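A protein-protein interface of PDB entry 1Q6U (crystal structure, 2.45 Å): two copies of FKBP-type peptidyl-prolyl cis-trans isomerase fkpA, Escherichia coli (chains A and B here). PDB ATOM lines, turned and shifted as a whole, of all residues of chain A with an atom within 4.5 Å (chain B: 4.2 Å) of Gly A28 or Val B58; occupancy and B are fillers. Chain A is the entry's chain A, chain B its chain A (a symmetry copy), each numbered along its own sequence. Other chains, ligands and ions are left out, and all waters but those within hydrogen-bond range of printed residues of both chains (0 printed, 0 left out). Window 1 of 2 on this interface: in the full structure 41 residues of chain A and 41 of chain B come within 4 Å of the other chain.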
ATOM      1  N   ALA A  24      -1.545  23.790   5.511  1.00  0.00           N
ATOM      2  CA  ALA A  24      -0.156  23.488   5.771  1.00  0.00           C
ATOM      3  C   ALA A  24       0.194  22.132   5.114  1.00  0.00           C
ATOM      4  O   ALA A  24       1.220  21.992   4.437  1.00  0.00           O
ATOM      5  CB  ALA A  24       0.100  23.455   7.249  1.00  0.00           C
ATOM      6  N   TYR A  25      -0.701  21.170   5.307  1.00  0.00           N
ATOM      7  CA  TYR A  25      -0.497  19.814   4.842  1.00  0.00           C
ATOM      8  C   TYR A  25      -0.509  19.814   3.339  1.00  0.00           C
ATOM      9  O   TYR A  25       0.342  19.209   2.707  1.00  0.00           O
ATOM     10  CB  TYR A  25      -1.587  18.918   5.414  1.00  0.00           C
ATOM     11  CG  TYR A  25      -1.457  17.463   5.111  1.00  0.00           C
ATOM     12  CD1 TYR A  25      -1.877  16.941   3.873  1.00  0.00           C
ATOM     13  CD2 TYR A  25      -0.963  16.588   6.070  1.00  0.00           C
ATOM     14  CE1 TYR A  25      -1.749  15.605   3.608  1.00  0.00           C
ATOM     15  CE2 TYR A  25      -0.827  15.229   5.814  1.00  0.00           C
ATOM     16  CZ  TYR A  25      -1.221  14.746   4.585  1.00  0.00           C
ATOM     17  OH  TYR A  25      -1.121  13.410   4.337  1.00  0.00           O
ATOM     18  N   ALA A  26      -1.441  20.544   2.762  1.00  0.00           N
ATOM     19  CA  ALA A  26      -1.483  20.592   1.318  1.00  0.00           C
ATOM     20  C   ALA A  26      -0.179  21.131   0.796  1.00  0.00           C
ATOM     21  O   ALA A  26       0.334  20.639  -0.187  1.00  0.00           O
ATOM     22  CB  ALA A  26      -2.591  21.435   0.841  1.00  0.00           C
ATOM     23  N   LEU A  27       0.329  22.156   1.445  1.00  0.00           N
ATOM     24  CA  LEU A  27       1.586  22.759   1.053  1.00  0.00           C
ATOM     25  C   LEU A  27       2.730  21.753   1.101  1.00  0.00           C
ATOM     26  O   LEU A  27       3.526  21.644   0.164  1.00  0.00           O
ATOM     27  CB  LEU A  27       1.921  23.961   1.932  1.00  0.00           C
ATOM     28  CG  LEU A  27       1.173  25.217   1.528  1.00  0.00           C
ATOM     29  CD1 LEU A  27       1.549  26.336   2.498  1.00  0.00           C
ATOM     30  CD2 LEU A  27       1.525  25.608   0.066  1.00  0.00           C
ATOM     31  N   GLY A  28       2.807  21.007   2.187  1.00  0.00           N
ATOM     32  CA  GLY A  28       3.827  19.983   2.309  1.00  0.00           C
ATOM     33  C   GLY A  28       3.675  18.883   1.283  1.00  0.00           C
ATOM     34  O   GLY A  28       4.619  18.425   0.691  1.00  0.00           O
ATOM     35  N   ALA A  29       2.440  18.466   1.089  1.00  0.00           N
ATOM     36  CA  ALA A  29       2.165  17.407   0.178  1.00  0.00           C
ATOM     37  C   ALA A  29       2.647  17.806  -1.171  1.00  0.00           C
ATOM     38  O   ALA A  29       3.230  16.979  -1.858  1.00  0.00           O
ATOM     39  CB  ALA A  29       0.685  17.090   0.138  1.00  0.00           C
ATOM     40  N   SER A  30       2.411  19.056  -1.565  1.00  0.00           N
ATOM     41  CA  SER A  30       2.767  19.439  -2.929  1.00  0.00           C
ATOM     42  C   SER A  30       4.268  19.487  -3.065  1.00  0.00           C
ATOM     43  O   SER A  30       4.810  19.174  -4.114  1.00  0.00           O
ATOM     44  CB  SER A  30       2.134  20.746  -3.385  1.00  0.00           C
ATOM     45  OG  SER A  30       2.988  21.825  -3.179  1.00  0.00           O
ATOM     46  N   LEU A  31       4.943  19.846  -1.994  1.00  0.00           N
ATOM     47  CA  LEU A  31       6.366  19.819  -2.044  1.00  0.00           C
ATOM     48  C   LEU A  31       6.904  18.371  -2.023  1.00  0.00           C
ATOM     49  O   LEU A  31       7.855  18.045  -2.738  1.00  0.00           O
ATOM     50  CB  LEU A  31       6.920  20.725  -0.964  1.00  0.00           C
ATOM     51  CG  LEU A  31       7.110  22.181  -1.501  1.00  0.00           C
ATOM     52  CD1 LEU A  31       6.206  22.616  -2.683  1.00  0.00           C
ATOM     53  CD2 LEU A  31       6.921  23.197  -0.389  1.00  0.00           C
ATOM     54  N   GLY A  32       6.294  17.511  -1.215  1.00  0.00           N
ATOM     55  CA  GLY A  32       6.663  16.116  -1.174  1.00  0.00           C
ATOM     56  C   GLY A  32       6.485  15.455  -2.553  1.00  0.00           C
ATOM     57  O   GLY A  32       7.297  14.671  -3.001  1.00  0.00           O
ATOM     58  N   ILE A  55      14.718  13.861   3.498  1.00  0.00           N
ATOM     59  CA  ILE A  55      13.760  14.287   4.506  1.00  0.00           C
ATOM     60  C   ILE A  55      14.482  14.890   5.715  1.00  0.00           C
ATOM     61  O   ILE A  55      14.013  15.838   6.313  1.00  0.00           O
ATOM     62  CB  ILE A  55      12.891  13.089   4.890  1.00  0.00           C
ATOM     63  CG1 ILE A  55      12.061  12.661   3.680  1.00  0.00           C
ATOM     64  CG2 ILE A  55      11.991  13.379   6.056  1.00  0.00           C
ATOM     65  CD1 ILE A  55      11.187  13.710   3.117  1.00  0.00           C
ATOM     66  N   LEU B  54       2.654  20.641   8.039  1.00  0.00           N
ATOM     67  CA  LEU B  54       3.432  20.918   6.857  1.00  0.00           C
ATOM     68  C   LEU B  54       4.444  19.801   6.624  1.00  0.00           C
ATOM     69  O   LEU B  54       4.570  19.243   5.537  1.00  0.00           O
ATOM     70  CB  LEU B  54       4.100  22.263   7.045  1.00  0.00           C
ATOM     71  CG  LEU B  54       4.935  22.865   5.937  1.00  0.00           C
ATOM     72  CD1 LEU B  54       4.164  23.229   4.717  1.00  0.00           C
ATOM     73  CD2 LEU B  54       5.544  24.105   6.510  1.00  0.00           C
ATOM     74  N   ILE B  55       5.140  19.419   7.672  1.00  0.00           N
ATOM     75  CA  ILE B  55       6.096  18.331   7.541  1.00  0.00           C
ATOM     76  C   ILE B  55       5.371  17.005   7.289  1.00  0.00           C
ATOM     77  O   ILE B  55       5.841  16.170   6.543  1.00  0.00           O
ATOM     78  CB  ILE B  55       6.960  18.287   8.801  1.00  0.00           C
ATOM     79  CG1 ILE B  55       7.793  19.566   8.885  1.00  0.00           C
ATOM     80  CG2 ILE B  55       7.857  17.084   8.844  1.00  0.00           C
ATOM     81  CD1 ILE B  55       8.671  19.819   7.725  1.00  0.00           C
ATOM     82  N   ALA B  56       4.211  16.825   7.897  1.00  0.00           N
ATOM     83  CA  ALA B  56       3.484  15.578   7.722  1.00  0.00           C
ATOM     84  C   ALA B  56       3.053  15.435   6.259  1.00  0.00           C
ATOM     85  O   ALA B  56       3.067  14.378   5.731  1.00  0.00           O
ATOM     86  CB  ALA B  56       2.317  15.486   8.690  1.00  0.00           C
ATOM     87  N   GLY B  57       2.712  16.518   5.600  1.00  0.00           N
ATOM     88  CA  GLY B  57       2.367  16.471   4.198  1.00  0.00           C
ATOM     89  C   GLY B  57       3.552  16.068   3.359  1.00  0.00           C
ATOM     90  O   GLY B  57       3.445  15.231   2.481  1.00  0.00           O
ATOM     91  N   VAL B  58       4.701  16.659   3.625  1.00  0.00           N
ATOM     92  CA  VAL B  58       5.890  16.302   2.904  1.00  0.00           C
ATOM     93  C   VAL B  58       6.131  14.809   3.106  1.00  0.00           C
ATOM     94  O   VAL B  58       6.257  14.073   2.152  1.00  0.00           O
ATOM     95  CB  VAL B  58       7.115  17.054   3.390  1.00  0.00           C
ATOM     96  CG1 VAL B  58       8.350  16.537   2.676  1.00  0.00           C
ATOM     97  CG2 VAL B  58       6.992  18.576   3.203  1.00  0.00           C
ATOM     98  N   GLN B  59       6.171  14.341   4.333  1.00  0.00           N
ATOM     99  CA  GLN B  59       6.384  12.926   4.551  1.00  0.00           C
ATOM    100  C   GLN B  59       5.344  11.991   3.895  1.00  0.00           C
ATOM    101  O   GLN B  59       5.697  11.050   3.184  1.00  0.00           O
ATOM    102  CB  GLN B  59       6.456  12.646   6.020  1.00  0.00           C
ATOM    103  CG  GLN B  59       7.623  13.339   6.689  1.00  0.00           C
ATOM    104  CD  GLN B  59       7.541  13.255   8.214  1.00  0.00           C
ATOM    105  OE1 GLN B  59       8.557  13.162   8.882  1.00  0.00           O
ATOM    106  NE2 GLN B  59       6.324  13.281   8.748  1.00  0.00           N
ATOM    107  N   ASP B  60       4.072  12.253   4.119  1.00  0.00           N
ATOM    108  CA  ASP B  60       3.038  11.393   3.583  1.00  0.00           C
ATOM    109  C   ASP B  60       3.124  11.267   2.070  1.00  0.00           C
ATOM    110  O   ASP B  60       3.103  10.200   1.541  1.00  0.00           O
ATOM    111  CB  ASP B  60       1.672  11.922   3.998  1.00  0.00           C
ATOM    112  CG  ASP B  60       1.362  11.682   5.498  1.00  0.00           C
ATOM    113  OD1 ASP B  60       2.194  11.068   6.221  1.00  0.00           O
ATOM    114  OD2 ASP B  60       0.292  12.068   6.037  1.00  0.00           O
ATOM    115  N   ALA B  61       3.257  12.378   1.381  1.00  0.00           N
ATOM    116  CA  ALA B  61       3.274  12.378  -0.067  1.00  0.00           C
ATOM    117  C   ALA B  61       4.498  11.690  -0.610  1.00  0.00           C
ATOM    118  O   ALA B  61       4.443  10.983  -1.607  1.00  0.00           O
ATOM    119  CB  ALA B  61       3.229  13.806  -0.577  1.00  0.00           C
ATOM    120  N   PHE B  62       5.614  11.916   0.060  1.00  0.00           N
ATOM    121  CA  PHE B  62       6.833  11.305  -0.326  1.00  0.00           C
ATOM    122  C   PHE B  62       6.730   9.824  -0.191  1.00  0.00           C
ATOM    123  O   PHE B  62       7.310   9.101  -0.987  1.00  0.00           O
ATOM    124  CB  PHE B  62       7.964  11.789   0.548  1.00  0.00           C
ATOM    125  CG  PHE B  62       9.245  11.782  -0.142  1.00  0.00           C
ATOM    126  CD1 PHE B  62       9.454  12.647  -1.198  1.00  0.00           C
ATOM    127  CD2 PHE B  62      10.216  10.888   0.206  1.00  0.00           C
ATOM    128  CE1 PHE B  62      10.617  12.636  -1.889  1.00  0.00           C
ATOM    129  CE2 PHE B  62      11.424  10.858  -0.496  1.00  0.00           C
ATOM    130  CZ  PHE B  62      11.621  11.732  -1.537  1.00  0.00           C
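Val B58 touches just these residues of chain A: Gly A28, Ala A29 and Gly A32.
Printed residues of chain B within 4 Å of Gly A32: Val B58 and Phe B62.
Printed residues of chain A within 4 Å of Leu B54: Ala A24, Leu A27 and Gly A28.
Of the printed residues of chain A, Asp B60 touches Tyr A25 (2.6 Å).
Of the printed residues of chain A, Gly B57 touches Tyr A25 (3.7 Å), Gly A28 (3.5 Å) and Ala A29 (3.4 Å).
Of the printed residues of chain B, Ala A24 touches Leu B54.
Ser A30 touches none of the printed residues of chain B.
The nearest printed residue of chain B that does not touch Gly A28 is Ala B61 (5.0 Å).
The nearest residue of chain A that does not touch Val B58 is Ile A55 (4.03 Å).
O of Leu A27 is in hydrogen-bond range of OG of Ser A30 (3.4 Å).
Along chain B the printed residues that touch a printed residue of chain A span positions 54 to 62.
Hydrophobic or aromatic side chains of chain A that line the printed part of chain B: Ala A24, Tyr A25 and Leu A27.
Among the printed residues, no Asp or Glu carboxylate lies within 4 Å of a Lys or Arg side-chain nitrogen of the other chain.
Among the printed residues, merely in contact across the chains: Ala A24 with Leu B54, Gly A28 with Leu B54, Ala A29 with Gly B57, Ala A29 with Ala B61, Gly A32 with Phe B62, Gly A28 with Gly B57, Leu A27 with Leu B54, Tyr A25 with Gly B57, Ala A29 with Val B58, Tyr A25 with Ala B56 and Gly A32 with Val B58.
Position printed for both chains: 55.
Of the 13 pairs that touch across the chains among the printed residues, none has its exchanged pair printed and touching as well.
The backbone carbonyl oxygen of Gly A28 sits close to the backbone NH of Val B58.
OH of Tyr A25 lies within hydrogen-bond range of OD2 of Asp B60 (2.6 Å).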
